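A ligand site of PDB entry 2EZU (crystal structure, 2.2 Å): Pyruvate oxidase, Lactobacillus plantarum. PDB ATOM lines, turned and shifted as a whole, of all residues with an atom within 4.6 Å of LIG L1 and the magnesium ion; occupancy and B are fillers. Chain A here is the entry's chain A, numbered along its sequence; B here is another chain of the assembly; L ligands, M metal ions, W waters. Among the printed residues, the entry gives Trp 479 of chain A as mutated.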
ATOM      1  N   ASN A  92      14.438 -26.057  12.314  1.00  0.00           N
ATOM      2  CA  ASN A  92      15.165 -24.889  11.749  1.00  0.00           C
ATOM      3  C   ASN A  92      14.300 -23.678  11.599  1.00  0.00           C
ATOM      4  O   ASN A  92      14.778 -22.545  11.801  1.00  0.00           O
ATOM      5  CB  ASN A  92      15.915 -25.198  10.447  1.00  0.00           C
ATOM      6  CG  ASN A  92      17.270 -25.818  10.708  1.00  0.00           C
ATOM      7  OD1 ASN A  92      17.359 -26.788  11.463  1.00  0.00           O
ATOM      8  ND2 ASN A  92      18.342 -25.252  10.120  1.00  0.00           N
ATOM      9  N   VAL A 394      20.482 -17.208   2.659  1.00  0.00           N
ATOM     10  CA  VAL A 394      21.565 -16.898   3.581  1.00  0.00           C
ATOM     11  C   VAL A 394      22.912 -17.261   2.952  1.00  0.00           C
ATOM     12  O   VAL A 394      23.124 -18.389   2.479  1.00  0.00           O
ATOM     13  CB  VAL A 394      21.367 -17.692   4.924  1.00  0.00           C
ATOM     14  CG1 VAL A 394      22.639 -17.703   5.765  1.00  0.00           C
ATOM     15  CG2 VAL A 394      20.192 -17.126   5.713  1.00  0.00           C
ATOM     16  N   GLY A 395      23.839 -16.304   2.972  1.00  0.00           N
ATOM     17  CA  GLY A 395      25.123 -16.477   2.308  1.00  0.00           C
ATOM     18  C   GLY A 395      25.537 -15.157   1.633  1.00  0.00           C
ATOM     19  O   GLY A 395      25.170 -14.071   2.110  1.00  0.00           O
ATOM     20  N   ASP A 396      26.283 -15.268   0.524  1.00  0.00           N
ATOM     21  CA  ASP A 396      26.710 -14.063  -0.217  1.00  0.00           C
ATOM     22  C   ASP A 396      25.537 -13.180  -0.641  1.00  0.00           C
ATOM     23  O   ASP A 396      25.705 -11.982  -0.767  1.00  0.00           O
ATOM     24  CB  ASP A 396      27.503 -14.413  -1.468  1.00  0.00           C
ATOM     25  CG  ASP A 396      28.992 -14.601  -1.215  1.00  0.00           C
ATOM     26  OD1 ASP A 396      29.484 -14.300  -0.113  1.00  0.00           O
ATOM     27  OD2 ASP A 396      29.691 -15.039  -2.171  1.00  0.00           O
ATOM     28  N   ILE A 397      24.366 -13.776  -0.881  1.00  0.00           N
ATOM     29  CA  ILE A 397      23.178 -13.021  -1.299  1.00  0.00           C
ATOM     30  C   ILE A 397      22.771 -11.923  -0.292  1.00  0.00           C
ATOM     31  O   ILE A 397      22.263 -10.883  -0.691  1.00  0.00           O
ATOM     32  CB  ILE A 397      21.949 -13.932  -1.637  1.00  0.00           C
ATOM     33  CG1 ILE A 397      20.822 -13.077  -2.250  1.00  0.00           C
ATOM     34  CG2 ILE A 397      21.424 -14.714  -0.379  1.00  0.00           C
ATOM     35  CD1 ILE A 397      21.197 -12.346  -3.574  1.00  0.00           C
ATOM     36  N   ALA A 420      19.989 -17.318  11.137  1.00  0.00           N
ATOM     37  CA  ALA A 420      20.646 -17.323   9.826  1.00  0.00           C
ATOM     38  C   ALA A 420      20.658 -18.752   9.247  1.00  0.00           C
ATOM     39  O   ALA A 420      21.704 -19.243   8.788  1.00  0.00           O
ATOM     40  CB  ALA A 420      22.063 -16.795   9.954  1.00  0.00           C
ATOM     41  N   THR A 421      19.498 -19.416   9.290  1.00  0.00           N
ATOM     42  CA  THR A 421      19.338 -20.693   8.598  1.00  0.00           C
ATOM     43  C   THR A 421      19.173 -20.564   7.095  1.00  0.00           C
ATOM     44  O   THR A 421      18.288 -19.846   6.593  1.00  0.00           O
ATOM     45  CB  THR A 421      18.173 -21.564   9.179  1.00  0.00           C
ATOM     46  OG1 THR A 421      18.119 -22.807   8.474  1.00  0.00           O
ATOM     47  CG2 THR A 421      16.764 -20.854   9.065  1.00  0.00           C
ATOM     48  N   MET A 422      20.030 -21.277   6.356  1.00  0.00           N
ATOM     49  CA  MET A 422      19.915 -21.449   4.923  1.00  0.00           C
ATOM     50  C   MET A 422      18.608 -22.155   4.579  1.00  0.00           C
ATOM     51  O   MET A 422      18.070 -22.904   5.406  1.00  0.00           O
ATOM     52  CB  MET A 422      21.088 -22.295   4.425  1.00  0.00           C
ATOM     53  CG  MET A 422      22.460 -21.574   4.387  1.00  0.00           C
ATOM     54  SD  MET A 422      23.813 -22.744   4.117  1.00  0.00           S
ATOM     55  CE  MET A 422      23.453 -23.280   2.431  1.00  0.00           C
ATOM     56  N   GLY A 446      21.256 -18.326  -2.827  1.00  0.00           N
ATOM     57  CA  GLY A 446      22.450 -19.038  -3.331  1.00  0.00           C
ATOM     58  C   GLY A 446      22.084 -20.472  -3.664  1.00  0.00           C
ATOM     59  O   GLY A 446      21.015 -20.981  -3.238  1.00  0.00           O
ATOM     60  N   ASP A 447      22.962 -21.136  -4.424  1.00  0.00           N
ATOM     61  CA  ASP A 447      22.743 -22.523  -4.801  1.00  0.00           C
ATOM     62  C   ASP A 447      22.783 -23.477  -3.606  1.00  0.00           C
ATOM     63  O   ASP A 447      21.999 -24.431  -3.559  1.00  0.00           O
ATOM     64  CB  ASP A 447      23.694 -22.995  -5.920  1.00  0.00           C
ATOM     65  CG  ASP A 447      25.177 -22.723  -5.643  1.00  0.00           C
ATOM     66  OD1 ASP A 447      25.604 -22.175  -4.599  1.00  0.00           O
ATOM     67  OD2 ASP A 447      25.968 -23.067  -6.554  1.00  0.00           O
ATOM     68  N   GLY A 448      23.676 -23.202  -2.650  1.00  0.00           N
ATOM     69  CA  GLY A 448      23.703 -23.970  -1.401  1.00  0.00           C
ATOM     70  C   GLY A 448      22.385 -23.929  -0.641  1.00  0.00           C
ATOM     71  O   GLY A 448      21.868 -24.961  -0.235  1.00  0.00           O
ATOM     72  N   GLY A 449      21.845 -22.725  -0.426  1.00  0.00           N
ATOM     73  CA  GLY A 449      20.577 -22.592   0.320  1.00  0.00           C
ATOM     74  C   GLY A 449      19.348 -23.045  -0.454  1.00  0.00           C
ATOM     75  O   GLY A 449      18.458 -23.683   0.114  1.00  0.00           O
ATOM     76  N   MET A 452      18.883 -26.858  -0.238  1.00  0.00           N
ATOM     77  CA  MET A 452      18.322 -27.394   0.991  1.00  0.00           C
ATOM     78  C   MET A 452      16.788 -27.499   1.019  1.00  0.00           C
ATOM     79  O   MET A 452      16.253 -28.432   1.642  1.00  0.00           O
ATOM     80  CB  MET A 452      18.829 -26.552   2.153  1.00  0.00           C
ATOM     81  CG  MET A 452      20.318 -26.840   2.410  1.00  0.00           C
ATOM     82  SD  MET A 452      20.921 -25.939   3.829  1.00  0.00           S
ATOM     83  CE  MET A 452      22.573 -26.659   4.059  1.00  0.00           C
ATOM     84  N   PHE A 472      21.642 -18.061  -7.417  1.00  0.00           N
ATOM     85  CA  PHE A 472      23.003 -17.612  -7.715  1.00  0.00           C
ATOM     86  C   PHE A 472      23.959 -18.790  -7.618  1.00  0.00           C
ATOM     87  O   PHE A 472      24.429 -19.117  -6.513  1.00  0.00           O
ATOM     88  CB  PHE A 472      23.408 -16.480  -6.752  1.00  0.00           C
ATOM     89  CG  PHE A 472      22.557 -15.226  -6.904  1.00  0.00           C
ATOM     90  CD1 PHE A 472      21.235 -15.195  -6.433  1.00  0.00           C
ATOM     91  CD2 PHE A 472      23.071 -14.074  -7.524  1.00  0.00           C
ATOM     92  CE1 PHE A 472      20.420 -14.048  -6.602  1.00  0.00           C
ATOM     93  CE2 PHE A 472      22.277 -12.919  -7.673  1.00  0.00           C
ATOM     94  CZ  PHE A 472      20.948 -12.910  -7.212  1.00  0.00           C
ATOM     95  N   ASN A 474      27.184 -20.436  -7.950  1.00  0.00           N
ATOM     96  CA  ASN A 474      28.634 -20.373  -7.996  1.00  0.00           C
ATOM     97  C   ASN A 474      29.301 -21.738  -7.777  1.00  0.00           C
ATOM     98  O   ASN A 474      30.525 -21.830  -7.783  1.00  0.00           O
ATOM     99  CB  ASN A 474      29.180 -19.299  -7.043  1.00  0.00           C
ATOM    100  CG  ASN A 474      28.657 -19.439  -5.648  1.00  0.00           C
ATOM    101  OD1 ASN A 474      28.019 -20.425  -5.322  1.00  0.00           O
ATOM    102  ND2 ASN A 474      28.990 -18.481  -4.787  1.00  0.00           N
ATOM    103  N   GLN A 476      29.570 -23.098  -5.090  1.00  0.00           N
ATOM    104  CA  GLN A 476      30.305 -22.974  -3.825  1.00  0.00           C
ATOM    105  C   GLN A 476      29.361 -22.623  -2.702  1.00  0.00           C
ATOM    106  O   GLN A 476      28.283 -22.079  -2.924  1.00  0.00           O
ATOM    107  CB  GLN A 476      31.371 -21.853  -3.923  1.00  0.00           C
ATOM    108  CG  GLN A 476      32.386 -21.993  -5.065  1.00  0.00           C
ATOM    109  CD  GLN A 476      33.209 -20.707  -5.315  1.00  0.00           C
ATOM    110  OE1 GLN A 476      34.268 -20.749  -5.901  1.00  0.00           O
ATOM    111  NE2 GLN A 476      32.708 -19.572  -4.848  1.00  0.00           N
ATOM    112  N   TYR A 477      29.798 -22.897  -1.478  1.00  0.00           N
ATOM    113  CA  TYR A 477      29.364 -22.161  -0.317  1.00  0.00           C
ATOM    114  C   TYR A 477      30.321 -20.976  -0.235  1.00  0.00           C
ATOM    115  O   TYR A 477      31.288 -21.011   0.552  1.00  0.00           O
ATOM    116  CB  TYR A 477      29.497 -23.020   0.963  1.00  0.00           C
ATOM    117  CG  TYR A 477      28.634 -24.251   0.972  1.00  0.00           C
ATOM    118  CD1 TYR A 477      27.238 -24.138   0.790  1.00  0.00           C
ATOM    119  CD2 TYR A 477      29.196 -25.525   1.169  1.00  0.00           C
ATOM    120  CE1 TYR A 477      26.424 -25.278   0.764  1.00  0.00           C
ATOM    121  CE2 TYR A 477      28.389 -26.657   1.163  1.00  0.00           C
ATOM    122  CZ  TYR A 477      26.999 -26.524   0.950  1.00  0.00           C
ATOM    123  OH  TYR A 477      26.214 -27.635   0.953  1.00  0.00           O
ATOM    124  N   GLY A 478      30.075 -19.951  -1.039  1.00  0.00           N
ATOM    125  CA  GLY A 478      31.049 -18.838  -1.185  1.00  0.00           C
ATOM    126  C   GLY A 478      31.304 -18.090   0.125  1.00  0.00           C
ATOM    127  O   GLY A 478      32.476 -17.774   0.445  1.00  0.00           O
ATOM    128  N   TRP A 479      30.248 -17.830   0.883  1.00  0.00           N
ATOM    129  CA  TRP A 479      30.361 -17.153   2.188  1.00  0.00           C
ATOM    130  C   TRP A 479      31.393 -17.842   3.067  1.00  0.00           C
ATOM    131  O   TRP A 479      32.175 -17.173   3.751  1.00  0.00           O
ATOM    132  CB  TRP A 479      29.001 -17.184   2.901  1.00  0.00           C
ATOM    133  CG  TRP A 479      28.808 -16.250   4.072  1.00  0.00           C
ATOM    134  CD1 TRP A 479      28.701 -16.598   5.387  1.00  0.00           C
ATOM    135  CD2 TRP A 479      28.652 -14.822   4.012  1.00  0.00           C
ATOM    136  NE1 TRP A 479      28.488 -15.481   6.161  1.00  0.00           N
ATOM    137  CE2 TRP A 479      28.454 -14.371   5.350  1.00  0.00           C
ATOM    138  CE3 TRP A 479      28.678 -13.869   2.977  1.00  0.00           C
ATOM    139  CZ2 TRP A 479      28.283 -13.008   5.674  1.00  0.00           C
ATOM    140  CZ3 TRP A 479      28.507 -12.521   3.291  1.00  0.00           C
ATOM    141  CH2 TRP A 479      28.316 -12.104   4.640  1.00  0.00           C
ATOM    142  N   ILE A 480      31.378 -19.173   3.055  1.00  0.00           N
ATOM    143  CA  ILE A 480      32.296 -20.021   3.862  1.00  0.00           C
ATOM    144  C   ILE A 480      33.665 -20.193   3.216  1.00  0.00           C
ATOM    145  O   ILE A 480      34.680 -20.251   3.932  1.00  0.00           O
ATOM    146  CB  ILE A 480      31.664 -21.440   4.144  1.00  0.00           C
ATOM    147  CG1 ILE A 480      30.200 -21.296   4.622  1.00  0.00           C
ATOM    148  CG2 ILE A 480      32.500 -22.295   5.142  1.00  0.00           C
ATOM    149  CD1 ILE A 480      30.051 -20.402   5.863  1.00  0.00           C
ATOM    150  N   ILE B  32      28.645 -30.181   6.621  1.00  0.00           N
ATOM    151  CA  ILE B  32      28.696 -28.958   5.805  1.00  0.00           C
ATOM    152  C   ILE B  32      29.459 -27.952   6.637  1.00  0.00           C
ATOM    153  O   ILE B  32      29.167 -27.852   7.829  1.00  0.00           O
ATOM    154  CB  ILE B  32      27.262 -28.433   5.469  1.00  0.00           C
ATOM    155  CG1 ILE B  32      26.580 -29.362   4.443  1.00  0.00           C
ATOM    156  CG2 ILE B  32      27.318 -26.944   4.984  1.00  0.00           C
ATOM    157  CD1 ILE B  32      25.111 -29.057   4.085  1.00  0.00           C
ATOM    158  N   PRO B  33      30.483 -27.279   6.056  1.00  0.00           N
ATOM    159  CA  PRO B  33      31.324 -26.365   6.880  1.00  0.00           C
ATOM    160  C   PRO B  33      30.594 -25.064   7.245  1.00  0.00           C
ATOM    161  O   PRO B  33      29.525 -24.800   6.722  1.00  0.00           O
ATOM    162  CB  PRO B  33      32.525 -26.058   5.969  1.00  0.00           C
ATOM    163  CG  PRO B  33      31.944 -26.201   4.552  1.00  0.00           C
ATOM    164  CD  PRO B  33      30.927 -27.330   4.649  1.00  0.00           C
ATOM    165  N   GLY B  34      31.196 -24.274   8.137  1.00  0.00           N
ATOM    166  CA  GLY B  34      30.679 -22.959   8.518  1.00  0.00           C
ATOM    167  C   GLY B  34      31.796 -22.293   9.307  1.00  0.00           C
ATOM    168  O   GLY B  34      32.701 -22.977   9.767  1.00  0.00           O
ATOM    169  N   GLU B  59      22.448 -31.057   6.121  1.00  0.00           N
ATOM    170  CA  GLU B  59      23.060 -31.765   7.258  1.00  0.00           C
ATOM    171  C   GLU B  59      22.269 -32.957   7.774  1.00  0.00           C
ATOM    172  O   GLU B  59      22.879 -33.849   8.337  1.00  0.00           O
ATOM    173  CB  GLU B  59      23.454 -30.839   8.419  1.00  0.00           C
ATOM    174  CG  GLU B  59      24.417 -29.727   8.033  1.00  0.00           C
ATOM    175  CD  GLU B  59      23.702 -28.473   7.499  1.00  0.00           C
ATOM    176  OE1 GLU B  59      22.500 -28.552   7.101  1.00  0.00           O
ATOM    177  OE2 GLU B  59      24.353 -27.426   7.501  1.00  0.00           O
ATOM    178  N   SER B  82      27.486 -26.899  11.484  1.00  0.00           N
ATOM    179  CA  SER B  82      27.927 -25.612  12.051  1.00  0.00           C
ATOM    180  C   SER B  82      26.927 -25.106  13.130  1.00  0.00           C
ATOM    181  O   SER B  82      25.818 -25.660  13.278  1.00  0.00           O
ATOM    182  CB  SER B  82      28.108 -24.576  10.950  1.00  0.00           C
ATOM    183  OG  SER B  82      26.950 -24.606  10.139  1.00  0.00           O
ATOM    184  N   PRO B  85      21.761 -23.431  12.902  1.00  0.00           N
ATOM    185  CA  PRO B  85      21.030 -24.196  11.900  1.00  0.00           C
ATOM    186  C   PRO B  85      21.749 -25.441  11.323  1.00  0.00           C
ATOM    187  O   PRO B  85      21.091 -26.349  10.866  1.00  0.00           O
ATOM    188  CB  PRO B  85      20.786 -23.162  10.776  1.00  0.00           C
ATOM    189  CG  PRO B  85      21.829 -22.129  10.952  1.00  0.00           C
ATOM    190  CD  PRO B  85      22.002 -22.039  12.457  1.00  0.00           C
ATOM    191  N   GLY B  86      23.079 -25.483  11.334  1.00  0.00           N
ATOM    192  CA  GLY B  86      23.805 -26.648  10.804  1.00  0.00           C
ATOM    193  C   GLY B  86      23.493 -27.862  11.673  1.00  0.00           C
ATOM    194  O   GLY B  86      23.131 -28.927  11.177  1.00  0.00           O
ATOM    195  N   HIS B  89      19.763 -29.099  11.928  1.00  0.00           N
ATOM    196  CA  HIS B  89      19.447 -29.892  10.741  1.00  0.00           C
ATOM    197  C   HIS B  89      19.795 -31.378  10.919  1.00  0.00           C
ATOM    198  O   HIS B  89      19.281 -32.233  10.188  1.00  0.00           O
ATOM    199  CB  HIS B  89      20.176 -29.372   9.480  1.00  0.00           C
ATOM    200  CG  HIS B  89      19.349 -28.520   8.581  1.00  0.00           C
ATOM    201  ND1 HIS B  89      19.868 -27.910   7.450  1.00  0.00           N
ATOM    202  CD2 HIS B  89      18.034 -28.164   8.630  1.00  0.00           C
ATOM    203  CE1 HIS B  89      18.911 -27.239   6.841  1.00  0.00           C
ATOM    204  NE2 HIS B  89      17.791 -27.355   7.543  1.00  0.00           N
ATOM    205  N   PHE B 121      26.250 -13.252  16.504  1.00  0.00           N
ATOM    206  CA  PHE B 121      25.644 -13.854  15.334  1.00  0.00           C
ATOM    207  C   PHE B 121      25.651 -15.387  15.380  1.00  0.00           C
ATOM    208  O   PHE B 121      26.709 -16.008  15.636  1.00  0.00           O
ATOM    209  CB  PHE B 121      26.409 -13.354  14.093  1.00  0.00           C
ATOM    210  CG  PHE B 121      25.915 -13.917  12.800  1.00  0.00           C
ATOM    211  CD1 PHE B 121      24.739 -13.464  12.232  1.00  0.00           C
ATOM    212  CD2 PHE B 121      26.611 -14.917  12.165  1.00  0.00           C
ATOM    213  CE1 PHE B 121      24.267 -13.988  11.048  1.00  0.00           C
ATOM    214  CE2 PHE B 121      26.146 -15.449  10.951  1.00  0.00           C
ATOM    215  CZ  PHE B 121      24.985 -14.967  10.401  1.00  0.00           C
ATOM    216  N   GLN B 122      24.487 -15.992  15.100  1.00  0.00           N
ATOM    217  CA  GLN B 122      24.248 -17.459  15.237  1.00  0.00           C
ATOM    218  C   GLN B 122      24.792 -18.049  16.531  1.00  0.00           C
ATOM    219  O   GLN B 122      25.209 -19.216  16.547  1.00  0.00           O
ATOM    220  CB  GLN B 122      24.887 -18.272  14.086  1.00  0.00           C
ATOM    221  CG  GLN B 122      24.195 -18.127  12.810  1.00  0.00           C
ATOM    222  CD  GLN B 122      24.792 -18.994  11.721  1.00  0.00           C
ATOM    223  OE1 GLN B 122      26.013 -19.091  11.585  1.00  0.00           O
ATOM    224  NE2 GLN B 122      23.937 -19.596  10.926  1.00  0.00           N
HETATM  225  N1  LIG L   1      23.737 -24.947   7.381  1.00  0.00           N
HETATM  226  C1  LIG L   1      22.601 -24.213   7.522  1.00  0.00           C
HETATM  227  C2  LIG L   1      21.242 -24.865   7.498  1.00  0.00           C
HETATM  228  N2  LIG L   1      22.661 -22.876   7.703  1.00  0.00           N
HETATM  229  C3  LIG L   1      23.850 -22.223   7.750  1.00  0.00           C
HETATM  230  N3  LIG L   1      23.797 -20.886   7.963  1.00  0.00           N
HETATM  231  C4  LIG L   1      25.063 -22.937   7.587  1.00  0.00           C
HETATM  232  C5  LIG L   1      24.940 -24.337   7.399  1.00  0.00           C
HETATM  233  C6  LIG L   1      26.457 -22.278   7.600  1.00  0.00           C
HETATM  234  N4  LIG L   1      26.545 -21.322   6.453  1.00  0.00           N
HETATM  235  C7  LIG L   1      26.370 -19.954   6.527  1.00  0.00           C
HETATM  236  S1  LIG L   1      26.451 -19.197   4.947  1.00  0.00           S
HETATM  237  C8  LIG L   1      26.771 -20.732   4.177  1.00  0.00           C
HETATM  238  C9  LIG L   1      26.772 -21.772   5.155  1.00  0.00           C
HETATM  239  C10 LIG L   1      26.998 -23.223   4.754  1.00  0.00           C
HETATM  240  C11 LIG L   1      27.001 -20.758   2.683  1.00  0.00           C
HETATM  241  C12 LIG L   1      25.799 -20.379   1.818  1.00  0.00           C
HETATM  242  O1  LIG L   1      26.054 -20.956   0.533  1.00  0.00           O
HETATM  243  P1  LIG L   1      25.221 -20.542  -0.729  1.00  0.00           P
HETATM  244  O2  LIG L   1      25.558 -18.963  -0.902  1.00  0.00           O
HETATM  245  O3  LIG L   1      25.703 -21.245  -1.972  1.00  0.00           O
HETATM  246  O4  LIG L   1      23.755 -20.601  -0.393  1.00  0.00           O
HETATM  247  P2  LIG L   1      26.849 -18.266  -1.588  1.00  0.00           P
HETATM  248  O5  LIG L   1      26.142 -17.252  -2.484  1.00  0.00           O
HETATM  249  O6  LIG L   1      27.589 -17.630  -0.432  1.00  0.00           O
HETATM  250  O7  LIG L   1      27.678 -19.263  -2.356  1.00  0.00           O
HETATM  251  C13 LIG L   1      26.163 -19.006   7.697  1.00  0.00           C
HETATM  252  O8  LIG L   1      26.217 -19.438   8.842  1.00  0.00           O
HETATM  253  C14 LIG L   1      26.054 -17.506   7.494  1.00  0.00           C
HETATM  254  P1  LG2 L   2      16.721  -6.919  16.167  1.00  0.00           P
HETATM  255  O1  LG2 L   2      15.408  -7.603  15.853  1.00  0.00           O
HETATM  256  O2  LG2 L   2      17.833  -7.762  16.710  1.00  0.00           O
HETATM  257  O3  LG2 L   2      16.492  -5.741  17.239  1.00  0.00           O
HETATM  258  C1  LG2 L   2      15.416  -4.810  17.152  1.00  0.00           C
HETATM  259  C2  LG2 L   2      15.499  -3.938  18.380  1.00  0.00           C
HETATM  260  O4  LG2 L   2      14.459  -2.971  18.312  1.00  0.00           O
HETATM  261  C3  LG2 L   2      15.272  -4.705  19.683  1.00  0.00           C
HETATM  262  O5  LG2 L   2      16.305  -4.304  20.592  1.00  0.00           O
HETATM  263  C4  LG2 L   2      13.880  -4.292  20.141  1.00  0.00           C
HETATM  264  O6  LG2 L   2      13.746  -4.199  21.540  1.00  0.00           O
HETATM  265  C5  LG2 L   2      13.786  -2.897  19.591  1.00  0.00           C
HETATM  266  N1  LG2 L   2      12.424  -2.398  19.315  1.00  0.00           N
HETATM  267  C6  LG2 L   2      11.390  -3.090  18.766  1.00  0.00           C
HETATM  268  N2  LG2 L   2      10.348  -2.254  18.612  1.00  0.00           N
HETATM  269  C7  LG2 L   2      10.745  -1.013  19.061  1.00  0.00           C
HETATM  270  C8  LG2 L   2      10.111   0.222  19.167  1.00  0.00           C
HETATM  271  N3  LG2 L   2       8.803   0.377  18.762  1.00  0.00           N
HETATM  272  N4  LG2 L   2      10.805   1.280  19.658  1.00  0.00           N
HETATM  273  C9  LG2 L   2      12.084   1.154  20.072  1.00  0.00           C
HETATM  274  N5  LG2 L   2      12.726  -0.031  19.985  1.00  0.00           N
HETATM  275  C10 LG2 L   2      12.074  -1.118  19.484  1.00  0.00           C
HETATM  276  N6  LG2 L   2      23.612  -7.447  10.151  1.00  0.00           N
HETATM  277  C11 LG2 L   2      24.445  -6.376  10.019  1.00  0.00           C
HETATM  278  O7  LG2 L   2      23.997  -5.249  10.295  1.00  0.00           O
HETATM  279  N7  LG2 L   2      25.739  -6.561   9.604  1.00  0.00           N
HETATM  280  C12 LG2 L   2      26.172  -7.817   9.313  1.00  0.00           C
HETATM  281  O8  LG2 L   2      27.326  -8.001   8.920  1.00  0.00           O
HETATM  282  C13 LG2 L   2      25.318  -8.924   9.426  1.00  0.00           C
HETATM  283  N8  LG2 L   2      25.702 -10.214   9.167  1.00  0.00           N
HETATM  284  C14 LG2 L   2      24.741 -11.085   8.754  1.00  0.00           C
HETATM  285  C15 LG2 L   2      25.038 -12.176   7.938  1.00  0.00           C
HETATM  286  C16 LG2 L   2      24.041 -13.041   7.505  1.00  0.00           C
HETATM  287  C17 LG2 L   2      24.444 -14.212   6.630  1.00  0.00           C
HETATM  288  C18 LG2 L   2      22.710 -12.808   7.888  1.00  0.00           C
HETATM  289  C19 LG2 L   2      21.544 -13.700   7.478  1.00  0.00           C
HETATM  290  C20 LG2 L   2      22.413 -11.702   8.723  1.00  0.00           C
HETATM  291  C21 LG2 L   2      23.410 -10.838   9.146  1.00  0.00           C
HETATM  292  N9  LG2 L   2      23.169  -9.761   9.952  1.00  0.00           N
HETATM  293  C22 LG2 L   2      24.016  -8.704   9.840  1.00  0.00           C
HETATM  294  C23 LG2 L   2      21.827  -9.481  10.473  1.00  0.00           C
HETATM  295  C24 LG2 L   2      22.149  -9.538  12.012  1.00  0.00           C
HETATM  296  O9  LG2 L   2      22.545 -10.844  12.493  1.00  0.00           O
HETATM  297  C25 LG2 L   2      21.090  -9.021  13.011  1.00  0.00           C
HETATM  298  O10 LG2 L   2      19.851  -9.767  12.927  1.00  0.00           O
HETATM  299  C26 LG2 L   2      20.862  -7.498  12.859  1.00  0.00           C
HETATM  300  O11 LG2 L   2      22.083  -6.732  12.722  1.00  0.00           O
HETATM  301  C27 LG2 L   2      20.068  -6.967  14.053  1.00  0.00           C
HETATM  302  O12 LG2 L   2      19.175  -6.019  13.453  1.00  0.00           O
HETATM  303  P2  LG2 L   2      18.149  -5.105  14.277  1.00  0.00           P
HETATM  304  O13 LG2 L   2      18.819  -4.551  15.507  1.00  0.00           O
HETATM  305  O14 LG2 L   2      17.588  -4.202  13.222  1.00  0.00           O
HETATM  306  O15 LG2 L   2      17.102  -6.228  14.735  1.00  0.00           O
HETATM  307 MG    MG M   1      26.796 -20.792  -3.528  1.00  0.00          MG
HETATM  308  O   HOH W   1      25.897 -22.119  11.006  1.00  0.00           O
HETATM  309  O   HOH W   2      29.379 -19.117   8.890  1.00  0.00           O
HETATM  310  O   HOH W   3      25.477 -19.154  -4.216  1.00  0.00           O
HETATM  311  O   HOH W   4      26.291 -15.506  -4.692  1.00  0.00           O
HETATM  312  O   HOH W   5      23.812 -16.631  -1.359  1.00  0.00           O
HETATM  313  O   HOH W   6      22.226 -18.575  -0.112  1.00  0.00           O
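The side-chain carboxylate (OE2) of Glu 59 of chain B is in hydrogen-bond range of a nitrogen (N1) of LIG L1 (2.6 Å). The side-chain amide oxygen (OE1) of Gln 122 of chain B lies close to an oxygen (O8) of LIG L1 (2.8 Å). N3 of LIG L1 lies within hydrogen-bond range of O of Ala 420 (2.8 Å). The backbone NH of Gly 478 is in hydrogen-bond range of an oxygen (O6) of LIG L1. An oxygen (O4) of LIG L1 sits at hydrogen-bond distance from the backbone NH of Gly 449 (2.9 Å). An oxygen (O6) of LIG L1 lies within hydrogen-bond range of the backbone NH (N) of Asp 396 (2.9 Å). The backbone NH (N) of Gly 448 sits at hydrogen-bond distance from an oxygen (O4) of LIG L1 (3.4 Å). N of Trp 479 is in hydrogen-bond range of O6 of LIG L1 (3.0 Å). The backbone NH (N) of Met 422 lies within hydrogen-bond range of a nitrogen (N2) of LIG L1 (3.4 Å).
N of Asp 447 lies within hydrogen-bond range of O of Phe 472 (3.3 Å). OE1 of Glu 59 of chain B sits at hydrogen-bond distance from ND1 of His 89 of chain B (2.7 Å). The side-chain amide nitrogen of Gln 122 of chain B lies within hydrogen-bond range of the backbone carbonyl oxygen of Ala 420 (3.1 Å). N of His 89 of chain B lies close to OD1 of Asn 92 (3.4 Å). The side-chain amide nitrogen (ND2) of Asn 92 is in hydrogen-bond range of the backbone carbonyl oxygen (O) of Pro 85 of chain B (3.1 Å). OG1 of Thr 421 sits at hydrogen-bond distance from ND2 of Asn 92 (3.0 Å).
Residues that only touch LIG L1: Asn 92 (3.9 Å), Val 394 (3.4 Å), Gly 395 (3.8 Å), Thr 421 (3.9 Å), Gly 446 (3.6 Å), Met 452 (3.8 Å), Tyr 477 (3.4 Å), Ile 480 (3.5 Å), Ile 32 of chain B (3.7 Å), Pro 33 of chain B (3.6 Å), Ser 82 of chain B (3.4 Å), Pro 85 of chain B (3.4 Å), Gly 86 of chain B (3.8 Å) and His 89 of chain B (3.3 Å). Hydrophobic or aromatic side chains within 4 Å of LIG L1: Val 394, Met 422, Met 452, Tyr 477, Trp 479, Ile 480, Ile 32 of chain B, Pro 85 of chain B and His 89 of chain B. 26 residues have an atom within 4 Å of LIG L1: Asn 92, Val 394, Gly 395, Asp 396, Ala 420, Thr 421, Met 422, Gly 446, Asp 447, Gly 448, Gly 449, Met 452, Asn 474, Gln 476, Tyr 477, Gly 478, Trp 479, Ile 480, Ile 32 of chain B, Pro 33 of chain B, Glu 59 of chain B, Ser 82 of chain B, Pro 85 of chain B, Gly 86 of chain B, His 89 of chain B and Gln 122 of chain B. The nearest printed residue that does not touch LIG L1 is Phe 121 of chain B (4.005 Å).
Three residues have an atom within 4 Å of the magnesium ion: Asp 447, Asn 474 and Gln 476.
The magnesium ion is bound by O3 of LIG L1 (2.0 Å), O of Gln 476 (2.1 Å), OD1 of Asp 447 (2.1 Å), O7 of LIG L1 (2.1 Å), OD1 of Asn 474 (2.2 Å) and water W3 (2.2 Å).
Water W3 lies within hydrogen-bond range of the backbone carbonyl oxygen (O) of Phe 472 (2.5 Å), an oxygen (O5) of LIG L1 (2.7 Å) and the backbone NH (N) of Asp 447 (3.2 Å). Water W6 lies within hydrogen-bond range of O4 of LIG L1 (2.6 Å), O of Val 394 (2.7 Å) and N of Gly 446 (2.9 Å). Water W1 lies within hydrogen-bond range of OG of Ser 82 of chain B (2.8 Å), OE1 of Gln 122 of chain B (3.1 Å) and O8 of LIG L1 (3.5 Å).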
